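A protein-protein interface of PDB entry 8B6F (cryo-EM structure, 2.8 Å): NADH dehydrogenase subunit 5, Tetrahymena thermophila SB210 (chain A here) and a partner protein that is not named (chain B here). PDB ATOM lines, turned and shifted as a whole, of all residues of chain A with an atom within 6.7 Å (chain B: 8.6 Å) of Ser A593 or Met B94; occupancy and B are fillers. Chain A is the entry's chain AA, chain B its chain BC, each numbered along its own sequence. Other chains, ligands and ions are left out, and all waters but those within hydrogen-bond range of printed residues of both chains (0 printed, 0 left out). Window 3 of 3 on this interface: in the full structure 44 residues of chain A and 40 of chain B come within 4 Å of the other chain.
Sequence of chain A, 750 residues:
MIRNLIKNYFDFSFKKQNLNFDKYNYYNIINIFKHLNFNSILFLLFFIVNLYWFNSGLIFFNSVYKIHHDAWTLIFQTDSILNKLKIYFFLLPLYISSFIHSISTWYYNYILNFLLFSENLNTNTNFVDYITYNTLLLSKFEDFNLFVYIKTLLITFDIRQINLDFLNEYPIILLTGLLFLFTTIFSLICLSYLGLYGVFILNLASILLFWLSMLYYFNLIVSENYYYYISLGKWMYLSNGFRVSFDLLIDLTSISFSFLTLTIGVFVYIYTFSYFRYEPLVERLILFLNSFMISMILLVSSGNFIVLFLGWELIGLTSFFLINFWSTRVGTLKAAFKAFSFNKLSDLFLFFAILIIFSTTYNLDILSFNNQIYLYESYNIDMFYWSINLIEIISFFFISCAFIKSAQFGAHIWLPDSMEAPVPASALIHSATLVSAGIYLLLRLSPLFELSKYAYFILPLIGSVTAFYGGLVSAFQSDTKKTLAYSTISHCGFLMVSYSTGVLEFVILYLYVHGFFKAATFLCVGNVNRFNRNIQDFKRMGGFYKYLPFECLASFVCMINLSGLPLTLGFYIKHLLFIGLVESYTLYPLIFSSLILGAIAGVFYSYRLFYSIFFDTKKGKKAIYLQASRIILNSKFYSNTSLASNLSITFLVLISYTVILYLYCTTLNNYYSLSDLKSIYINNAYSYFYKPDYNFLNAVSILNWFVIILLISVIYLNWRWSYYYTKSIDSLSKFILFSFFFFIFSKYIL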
ATOM      1  N   VAL A 465      -0.956 -30.463  26.719  1.00  0.00           N
ATOM      2  CA  VAL A 465       0.223 -31.323  26.681  1.00  0.00           C
ATOM      3  C   VAL A 465      -0.161 -32.711  26.193  1.00  0.00           C
ATOM      4  O   VAL A 465       0.528 -33.306  25.357  1.00  0.00           O
ATOM      5  CB  VAL A 465       0.901 -31.370  28.063  1.00  0.00           C
ATOM      6  CG1 VAL A 465       1.981 -32.443  28.103  1.00  0.00           C
ATOM      7  CG2 VAL A 465       1.499 -30.018  28.405  1.00  0.00           C
ATOM      8  N   PHE A 468      -0.873 -32.578  22.360  1.00  0.00           N
ATOM      9  CA  PHE A 468       0.344 -32.570  21.559  1.00  0.00           C
ATOM     10  C   PHE A 468       1.027 -33.931  21.587  1.00  0.00           C
ATOM     11  O   PHE A 468       1.381 -34.486  20.541  1.00  0.00           O
ATOM     12  CB  PHE A 468       1.292 -31.482  22.066  1.00  0.00           C
ATOM     13  CG  PHE A 468       2.728 -31.711  21.695  1.00  0.00           C
ATOM     14  CD1 PHE A 468       3.208 -31.324  20.458  1.00  0.00           C
ATOM     15  CD2 PHE A 468       3.599 -32.302  22.593  1.00  0.00           C
ATOM     16  CE1 PHE A 468       4.527 -31.532  20.118  1.00  0.00           C
ATOM     17  CE2 PHE A 468       4.919 -32.513  22.258  1.00  0.00           C
ATOM     18  CZ  PHE A 468       5.384 -32.126  21.019  1.00  0.00           C
ATOM     19  N   TYR A 588       0.132 -19.748  28.777  1.00  0.00           N
ATOM     20  CA  TYR A 588      -0.551 -19.676  27.489  1.00  0.00           C
ATOM     21  C   TYR A 588       0.364 -19.958  26.306  1.00  0.00           C
ATOM     22  O   TYR A 588      -0.080 -20.648  25.373  1.00  0.00           O
ATOM     23  CB  TYR A 588      -1.208 -18.299  27.336  1.00  0.00           C
ATOM     24  CG  TYR A 588      -1.924 -18.114  26.021  1.00  0.00           C
ATOM     25  CD1 TYR A 588      -3.180 -18.665  25.808  1.00  0.00           C
ATOM     26  CD2 TYR A 588      -1.341 -17.391  24.988  1.00  0.00           C
ATOM     27  CE1 TYR A 588      -3.839 -18.499  24.606  1.00  0.00           C
ATOM     28  CE2 TYR A 588      -1.991 -17.219  23.784  1.00  0.00           C
ATOM     29  CZ  TYR A 588      -3.240 -17.775  23.599  1.00  0.00           C
ATOM     30  OH  TYR A 588      -3.892 -17.606  22.400  1.00  0.00           O
ATOM     31  N   PRO A 589       1.609 -19.478  26.263  1.00  0.00           N
ATOM     32  CA  PRO A 589       2.471 -19.824  25.119  1.00  0.00           C
ATOM     33  C   PRO A 589       2.591 -21.320  24.907  1.00  0.00           C
ATOM     34  O   PRO A 589       2.340 -21.812  23.800  1.00  0.00           O
ATOM     35  CB  PRO A 589       3.813 -19.178  25.493  1.00  0.00           C
ATOM     36  CG  PRO A 589       3.461 -18.078  26.423  1.00  0.00           C
ATOM     37  CD  PRO A 589       2.279 -18.562  27.203  1.00  0.00           C
ATOM     38  N   LEU A 590       2.974 -22.064  25.946  1.00  0.00           N
ATOM     39  CA  LEU A 590       3.097 -23.510  25.810  1.00  0.00           C
ATOM     40  C   LEU A 590       1.755 -24.143  25.470  1.00  0.00           C
ATOM     41  O   LEU A 590       1.679 -25.039  24.622  1.00  0.00           O
ATOM     42  CB  LEU A 590       3.662 -24.106  27.098  1.00  0.00           C
ATOM     43  CG  LEU A 590       3.791 -25.629  27.154  1.00  0.00           C
ATOM     44  CD1 LEU A 590       4.789 -26.126  26.123  1.00  0.00           C
ATOM     45  CD2 LEU A 590       4.194 -26.070  28.546  1.00  0.00           C
ATOM     46  N   ILE A 591       0.687 -23.698  26.133  1.00  0.00           N
ATOM     47  CA  ILE A 591      -0.632 -24.278  25.892  1.00  0.00           C
ATOM     48  C   ILE A 591      -1.021 -24.119  24.429  1.00  0.00           C
ATOM     49  O   ILE A 591      -1.456 -25.073  23.775  1.00  0.00           O
ATOM     50  CB  ILE A 591      -1.677 -23.640  26.828  1.00  0.00           C
ATOM     51  CG1 ILE A 591      -1.403 -24.047  28.277  1.00  0.00           C
ATOM     52  CG2 ILE A 591      -3.091 -24.053  26.424  1.00  0.00           C
ATOM     53  CD1 ILE A 591      -2.197 -23.263  29.297  1.00  0.00           C
ATOM     54  N   PHE A 592      -0.872 -22.907  23.893  1.00  0.00           N
ATOM     55  CA  PHE A 592      -1.299 -22.654  22.522  1.00  0.00           C
ATOM     56  C   PHE A 592      -0.422 -23.391  21.517  1.00  0.00           C
ATOM     57  O   PHE A 592      -0.931 -23.966  20.549  1.00  0.00           O
ATOM     58  CB  PHE A 592      -1.291 -21.153  22.246  1.00  0.00           C
ATOM     59  CG  PHE A 592      -1.978 -20.776  20.971  1.00  0.00           C
ATOM     60  CD1 PHE A 592      -3.342 -20.545  20.949  1.00  0.00           C
ATOM     61  CD2 PHE A 592      -1.261 -20.651  19.795  1.00  0.00           C
ATOM     62  CE1 PHE A 592      -3.980 -20.200  19.776  1.00  0.00           C
ATOM     63  CE2 PHE A 592      -1.891 -20.307  18.620  1.00  0.00           C
ATOM     64  CZ  PHE A 592      -3.253 -20.079  18.609  1.00  0.00           C
ATOM     65  N   SER A 593       0.895 -23.389  21.727  1.00  0.00           N
ATOM     66  CA  SER A 593       1.785 -24.097  20.811  1.00  0.00           C
ATOM     67  C   SER A 593       1.496 -25.592  20.811  1.00  0.00           C
ATOM     68  O   SER A 593       1.465 -26.227  19.751  1.00  0.00           O
ATOM     69  CB  SER A 593       3.243 -23.827  21.179  1.00  0.00           C
ATOM     70  OG  SER A 593       3.481 -24.100  22.549  1.00  0.00           O
ATOM     71  N   SER A 594       1.284 -26.174  21.994  1.00  0.00           N
ATOM     72  CA  SER A 594       0.955 -27.594  22.068  1.00  0.00           C
ATOM     73  C   SER A 594      -0.370 -27.888  21.376  1.00  0.00           C
ATOM     74  O   SER A 594      -0.504 -28.898  20.677  1.00  0.00           O
ATOM     75  CB  SER A 594       0.903 -28.042  23.529  1.00  0.00           C
ATOM     76  OG  SER A 594       2.109 -27.735  24.204  1.00  0.00           O
ATOM     77  N   LEU A 595      -1.364 -27.017  21.564  1.00  0.00           N
ATOM     78  CA  LEU A 595      -2.648 -27.208  20.900  1.00  0.00           C
ATOM     79  C   LEU A 595      -2.501 -27.171  19.386  1.00  0.00           C
ATOM     80  O   LEU A 595      -3.098 -27.990  18.679  1.00  0.00           O
ATOM     81  CB  LEU A 595      -3.637 -26.140  21.364  1.00  0.00           C
ATOM     82  CG  LEU A 595      -4.268 -26.362  22.736  1.00  0.00           C
ATOM     83  CD1 LEU A 595      -5.078 -25.154  23.156  1.00  0.00           C
ATOM     84  CD2 LEU A 595      -5.147 -27.598  22.705  1.00  0.00           C
ATOM     85  N   ILE A 596      -1.723 -26.221  18.868  1.00  0.00           N
ATOM     86  CA  ILE A 596      -1.546 -26.123  17.421  1.00  0.00           C
ATOM     87  C   ILE A 596      -0.866 -27.378  16.889  1.00  0.00           C
ATOM     88  O   ILE A 596      -1.288 -27.954  15.880  1.00  0.00           O
ATOM     89  CB  ILE A 596      -0.753 -24.851  17.066  1.00  0.00           C
ATOM     90  CG1 ILE A 596      -1.568 -23.597  17.402  1.00  0.00           C
ATOM     91  CG2 ILE A 596      -0.343 -24.855  15.593  1.00  0.00           C
ATOM     92  CD1 ILE A 596      -2.835 -23.422  16.584  1.00  0.00           C
ATOM     93  N   LEU A 597       0.201 -27.818  17.560  1.00  0.00           N
ATOM     94  CA  LEU A 597       0.919 -29.003  17.105  1.00  0.00           C
ATOM     95  C   LEU A 597       0.026 -30.236  17.150  1.00  0.00           C
ATOM     96  O   LEU A 597       0.030 -31.051  16.220  1.00  0.00           O
ATOM     97  CB  LEU A 597       2.176 -29.213  17.948  1.00  0.00           C
ATOM     98  CG  LEU A 597       3.282 -28.166  17.775  1.00  0.00           C
ATOM     99  CD1 LEU A 597       4.437 -28.447  18.718  1.00  0.00           C
ATOM    100  CD2 LEU A 597       3.777 -28.105  16.336  1.00  0.00           C
ATOM    101  N   GLY A 598      -0.736 -30.400  18.229  1.00  0.00           N
ATOM    102  CA  GLY A 598      -1.642 -31.532  18.312  1.00  0.00           C
ATOM    103  C   GLY A 598      -2.712 -31.500  17.239  1.00  0.00           C
ATOM    104  O   GLY A 598      -3.050 -32.531  16.653  1.00  0.00           O
ATOM    105  N   SER B  87      13.581 -34.291  22.975  1.00  0.00           N
ATOM    106  CA  SER B  87      12.473 -33.365  23.163  1.00  0.00           C
ATOM    107  C   SER B  87      12.893 -31.911  23.022  1.00  0.00           C
ATOM    108  O   SER B  87      12.023 -31.041  22.914  1.00  0.00           O
ATOM    109  CB  SER B  87      11.843 -33.587  24.539  1.00  0.00           C
ATOM    110  OG  SER B  87      10.695 -32.773  24.709  1.00  0.00           O
ATOM    111  N   ALA B  88      14.196 -31.626  23.022  1.00  0.00           N
ATOM    112  CA  ALA B  88      14.662 -30.289  22.675  1.00  0.00           C
ATOM    113  C   ALA B  88      14.122 -29.853  21.320  1.00  0.00           C
ATOM    114  O   ALA B  88      13.800 -28.677  21.119  1.00  0.00           O
ATOM    115  CB  ALA B  88      16.189 -30.252  22.681  1.00  0.00           C
ATOM    116  N   TYR B  89      14.016 -30.788  20.375  1.00  0.00           N
ATOM    117  CA  TYR B  89      13.475 -30.453  19.062  1.00  0.00           C
ATOM    118  C   TYR B  89      12.027 -29.996  19.163  1.00  0.00           C
ATOM    119  O   TYR B  89      11.631 -29.018  18.519  1.00  0.00           O
ATOM    120  CB  TYR B  89      13.580 -31.652  18.124  1.00  0.00           C
ATOM    121  CG  TYR B  89      14.992 -32.112  17.857  1.00  0.00           C
ATOM    122  CD1 TYR B  89      15.885 -31.305  17.166  1.00  0.00           C
ATOM    123  CD2 TYR B  89      15.422 -33.364  18.269  1.00  0.00           C
ATOM    124  CE1 TYR B  89      17.173 -31.726  16.909  1.00  0.00           C
ATOM    125  CE2 TYR B  89      16.707 -33.794  18.017  1.00  0.00           C
ATOM    126  CZ  TYR B  89      17.578 -32.971  17.337  1.00  0.00           C
ATOM    127  OH  TYR B  89      18.860 -33.399  17.083  1.00  0.00           O
ATOM    128  N   TRP B  90      11.217 -30.695  19.958  1.00  0.00           N
ATOM    129  CA  TRP B  90       9.830 -30.283  20.132  1.00  0.00           C
ATOM    130  C   TRP B  90       9.737 -28.951  20.860  1.00  0.00           C
ATOM    131  O   TRP B  90       8.847 -28.147  20.563  1.00  0.00           O
ATOM    132  CB  TRP B  90       9.045 -31.358  20.880  1.00  0.00           C
ATOM    133  CG  TRP B  90       9.022 -32.669  20.164  1.00  0.00           C
ATOM    134  CD1 TRP B  90       9.530 -33.850  20.611  1.00  0.00           C
ATOM    135  CD2 TRP B  90       8.476 -32.931  18.867  1.00  0.00           C
ATOM    136  NE1 TRP B  90       9.330 -34.834  19.675  1.00  0.00           N
ATOM    137  CE2 TRP B  90       8.684 -34.295  18.594  1.00  0.00           C
ATOM    138  CE3 TRP B  90       7.828 -32.142  17.910  1.00  0.00           C
ATOM    139  CZ2 TRP B  90       8.267 -34.891  17.409  1.00  0.00           C
ATOM    140  CZ3 TRP B  90       7.414 -32.737  16.732  1.00  0.00           C
ATOM    141  CH2 TRP B  90       7.637 -34.098  16.491  1.00  0.00           C
ATOM    142  N   TRP B  91      10.642 -28.693  21.804  1.00  0.00           N
ATOM    143  CA  TRP B  91      10.677 -27.381  22.441  1.00  0.00           C
ATOM    144  C   TRP B  91      10.940 -26.293  21.410  1.00  0.00           C
ATOM    145  O   TRP B  91      10.303 -25.234  21.435  1.00  0.00           O
ATOM    146  CB  TRP B  91      11.751 -27.351  23.528  1.00  0.00           C
ATOM    147  CG  TRP B  91      11.544 -28.347  24.621  1.00  0.00           C
ATOM    148  CD1 TRP B  91      10.407 -29.050  24.889  1.00  0.00           C
ATOM    149  CD2 TRP B  91      12.510 -28.759  25.593  1.00  0.00           C
ATOM    150  NE1 TRP B  91      10.605 -29.873  25.970  1.00  0.00           N
ATOM    151  CE2 TRP B  91      11.889 -29.712  26.421  1.00  0.00           C
ATOM    152  CE3 TRP B  91      13.843 -28.413  25.843  1.00  0.00           C
ATOM    153  CZ2 TRP B  91      12.553 -30.325  27.482  1.00  0.00           C
ATOM    154  CZ3 TRP B  91      14.500 -29.019  26.897  1.00  0.00           C
ATOM    155  CH2 TRP B  91      13.855 -29.965  27.704  1.00  0.00           C
ATOM    156  N   ALA B  92      11.881 -26.535  20.497  1.00  0.00           N
ATOM    157  CA  ALA B  92      12.163 -25.565  19.446  1.00  0.00           C
ATOM    158  C   ALA B  92      10.953 -25.365  18.541  1.00  0.00           C
ATOM    159  O   ALA B  92      10.639 -24.233  18.154  1.00  0.00           O
ATOM    160  CB  ALA B  92      13.371 -26.018  18.630  1.00  0.00           C
ATOM    161  N   MET B  93      10.266 -26.452  18.184  1.00  0.00           N
ATOM    162  CA  MET B  93       9.066 -26.329  17.362  1.00  0.00           C
ATOM    163  C   MET B  93       8.013 -25.489  18.070  1.00  0.00           C
ATOM    164  O   MET B  93       7.401 -24.600  17.468  1.00  0.00           O
ATOM    165  CB  MET B  93       8.501 -27.711  17.036  1.00  0.00           C
ATOM    166  CG  MET B  93       9.208 -28.448  15.912  1.00  0.00           C
ATOM    167  SD  MET B  93       8.231 -29.866  15.380  1.00  0.00           S
ATOM    168  CE  MET B  93       9.333 -30.656  14.218  1.00  0.00           C
ATOM    169  N   MET B  94       7.787 -25.758  19.357  1.00  0.00           N
ATOM    170  CA  MET B  94       6.811 -24.981  20.113  1.00  0.00           C
ATOM    171  C   MET B  94       7.201 -23.513  20.168  1.00  0.00           C
ATOM    172  O   MET B  94       6.352 -22.629  20.007  1.00  0.00           O
ATOM    173  CB  MET B  94       6.674 -25.541  21.528  1.00  0.00           C
ATOM    174  CG  MET B  94       6.045 -26.920  21.600  1.00  0.00           C
ATOM    175  SD  MET B  94       6.002 -27.547  23.288  1.00  0.00           S
ATOM    176  CE  MET B  94       5.348 -29.189  23.021  1.00  0.00           C
ATOM    177  N   ALA B  95       8.484 -23.231  20.398  1.00  0.00           N
ATOM    178  CA  ALA B  95       8.932 -21.844  20.455  1.00  0.00           C
ATOM    179  C   ALA B  95       8.691 -21.136  19.130  1.00  0.00           C
ATOM    180  O   ALA B  95       8.206 -20.000  19.103  1.00  0.00           O
ATOM    181  CB  ALA B  95      10.411 -21.789  20.833  1.00  0.00           C
ATOM    182  N   MET B  96       9.021 -21.793  18.016  1.00  0.00           N
ATOM    183  CA  MET B  96       8.819 -21.171  16.711  1.00  0.00           C
ATOM    184  C   MET B  96       7.342 -20.932  16.434  1.00  0.00           C
ATOM    185  O   MET B  96       6.963 -19.870  15.927  1.00  0.00           O
ATOM    186  CB  MET B  96       9.436 -22.036  15.615  1.00  0.00           C
ATOM    187  CG  MET B  96      10.953 -22.072  15.647  1.00  0.00           C
ATOM    188  SD  MET B  96      11.672 -22.897  14.218  1.00  0.00           S
ATOM    189  CE  MET B  96      11.072 -24.565  14.449  1.00  0.00           C
ATOM    190  N   VAL B  97       6.488 -21.908  16.752  1.00  0.00           N
ATOM    191  CA  VAL B  97       5.056 -21.739  16.511  1.00  0.00           C
ATOM    192  C   VAL B  97       4.514 -20.582  17.342  1.00  0.00           C
ATOM    193  O   VAL B  97       3.758 -19.739  16.845  1.00  0.00           O
ATOM    194  CB  VAL B  97       4.299 -23.047  16.812  1.00  0.00           C
ATOM    195  CG1 VAL B  97       2.792 -22.819  16.804  1.00  0.00           C
ATOM    196  CG2 VAL B  97       4.669 -24.124  15.813  1.00  0.00           C
ATOM    197  N   PHE B  98       4.888 -20.525  18.620  1.00  0.00           N
ATOM    198  CA  PHE B  98       4.393 -19.452  19.476  1.00  0.00           C
ATOM    199  C   PHE B  98       4.898 -18.096  19.007  1.00  0.00           C
ATOM    200  O   PHE B  98       4.160 -17.104  19.042  1.00  0.00           O
ATOM    201  CB  PHE B  98       4.795 -19.688  20.928  1.00  0.00           C
ATOM    202  CG  PHE B  98       4.508 -18.517  21.819  1.00  0.00           C
ATOM    203  CD1 PHE B  98       3.203 -18.143  22.091  1.00  0.00           C
ATOM    204  CD2 PHE B  98       5.542 -17.775  22.363  1.00  0.00           C
ATOM    205  CE1 PHE B  98       2.932 -17.059  22.902  1.00  0.00           C
ATOM    206  CE2 PHE B  98       5.279 -16.686  23.175  1.00  0.00           C
ATOM    207  CZ  PHE B  98       3.972 -16.330  23.445  1.00  0.00           C
ATOM    208  N   GLY B  99       6.155 -18.027  18.569  1.00  0.00           N
ATOM    209  CA  GLY B  99       6.662 -16.775  18.038  1.00  0.00           C
ATOM    210  C   GLY B  99       5.910 -16.333  16.799  1.00  0.00           C
ATOM    211  O   GLY B  99       5.577 -15.156  16.652  1.00  0.00           O
ATOM    212  N   PHE B 100       5.629 -17.271  15.893  1.00  0.00           N
ATOM    213  CA  PHE B 100       4.881 -16.926  14.691  1.00  0.00           C
ATOM    214  C   PHE B 100       3.500 -16.387  15.040  1.00  0.00           C
ATOM    215  O   PHE B 100       3.041 -15.404  14.448  1.00  0.00           O
ATOM    216  CB  PHE B 100       4.766 -18.151  13.786  1.00  0.00           C
ATOM    217  CG  PHE B 100       4.184 -17.856  12.438  1.00  0.00           C
ATOM    218  CD1 PHE B 100       2.812 -17.812  12.257  1.00  0.00           C
ATOM    219  CD2 PHE B 100       5.007 -17.628  11.348  1.00  0.00           C
ATOM    220  CE1 PHE B 100       2.271 -17.542  11.016  1.00  0.00           C
ATOM    221  CE2 PHE B 100       4.473 -17.357  10.105  1.00  0.00           C
ATOM    222  CZ  PHE B 100       3.103 -17.313   9.938  1.00  0.00           C
ATOM    223  N   TYR B 101       2.821 -17.018  15.998  1.00  0.00           N
ATOM    224  CA  TYR B 101       1.501 -16.546  16.399  1.00  0.00           C
ATOM    225  C   TYR B 101       1.588 -15.257  17.205  1.00  0.00           C
ATOM    226  O   TYR B 101       0.638 -14.467  17.213  1.00  0.00           O
ATOM    227  CB  TYR B 101       0.778 -17.626  17.201  1.00  0.00           C
ATOM    228  CG  TYR B 101       0.004 -18.597  16.340  1.00  0.00           C
ATOM    229  CD1 TYR B 101      -1.305 -18.331  15.961  1.00  0.00           C
ATOM    230  CD2 TYR B 101       0.584 -19.782  15.907  1.00  0.00           C
ATOM    231  CE1 TYR B 101      -2.013 -19.219  15.175  1.00  0.00           C
ATOM    232  CE2 TYR B 101      -0.116 -20.675  15.122  1.00  0.00           C
ATOM    233  CZ  TYR B 101      -1.415 -20.388  14.760  1.00  0.00           C
ATOM    234  OH  TYR B 101      -2.116 -21.274  13.980  1.00  0.00           O
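Of the printed residues of chain B, Ser A593 touches Met B94 (3.5 Å).
Of chain A, only Phe A468 (3.4 Å), Leu A590 (3.4 Å), Ser A593 (3.5 Å), Ser A594 (3.7 Å) and Leu A597 (3.6 Å) come within 4 Å of Met B94.
Of the printed residues of chain B, Ser A594 touches Met B94 (3.7 Å).
Of the printed residues of chain A, Val B97 touches Ile A596.
Printed residues of chain B within 4 Å of Pro A589: Phe B98 (3.5 Å).
Gly A598 touches none of the printed residues of chain B.
The nearest residue of chain A that does not touch Met B94 is Pro A589 (5.6 Å).
Of the 13 printed residues of chain A, 8 touch a printed residue of chain B.
Printed residues of chain A that touch a printed residue of chain B: Phe A468, Pro A589, Leu A590, Phe A592, Ser A593, Ser A594, Ile A596 and Leu A597.
Of the 15 printed residues of chain B, 5 touch a printed residue of chain A.
Printed residues of chain B that touch a printed residue of chain A: Trp B90, Met B94, Val B97, Phe B98 and Tyr B101.
Hydrophobic or aromatic side chains of chain B that line the printed part of chain A: Trp B90, Met B94, Val B97, Phe B98 and Tyr B101.
Along chain B the printed residues that touch a printed residue of chain A span positions 90 to 101.
Among the printed residues, no Asp or Glu carboxylate lies within 4 Å of a Lys or Arg side-chain nitrogen of the other chain.
O of Pro A589 is in hydrogen-bond range of OG of Ser A593 (2.8 Å).
The backbone carbonyl oxygen of Leu A590 lies within hydrogen-bond range of the side-chain hydroxyl of Ser A593 (2.9 Å).
The backbone carbonyl oxygen (O) of Leu A590 sits at hydrogen-bond distance from the side-chain hydroxyl (OG) of Ser A594, 2.8 Å away.
Among the printed residues, merely in contact across the chains: Phe A468 with Trp B90 (3.7 Å), Phe A468 with Met B94 (3.4 Å), Pro A589 with Phe B98 (3.5 Å), Leu A590 with Met B94 (3.4 Å), Phe A592 with Tyr B101 (3.4 Å), Ser A593 with Met B94 (3.5 Å), Ser A594 with Met B94 (3.7 Å), Ile A596 with Val B97 (3.9 Å), Ile A596 with Tyr B101 (3.5 Å) and Leu A597 with Met B94 (3.6 Å).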
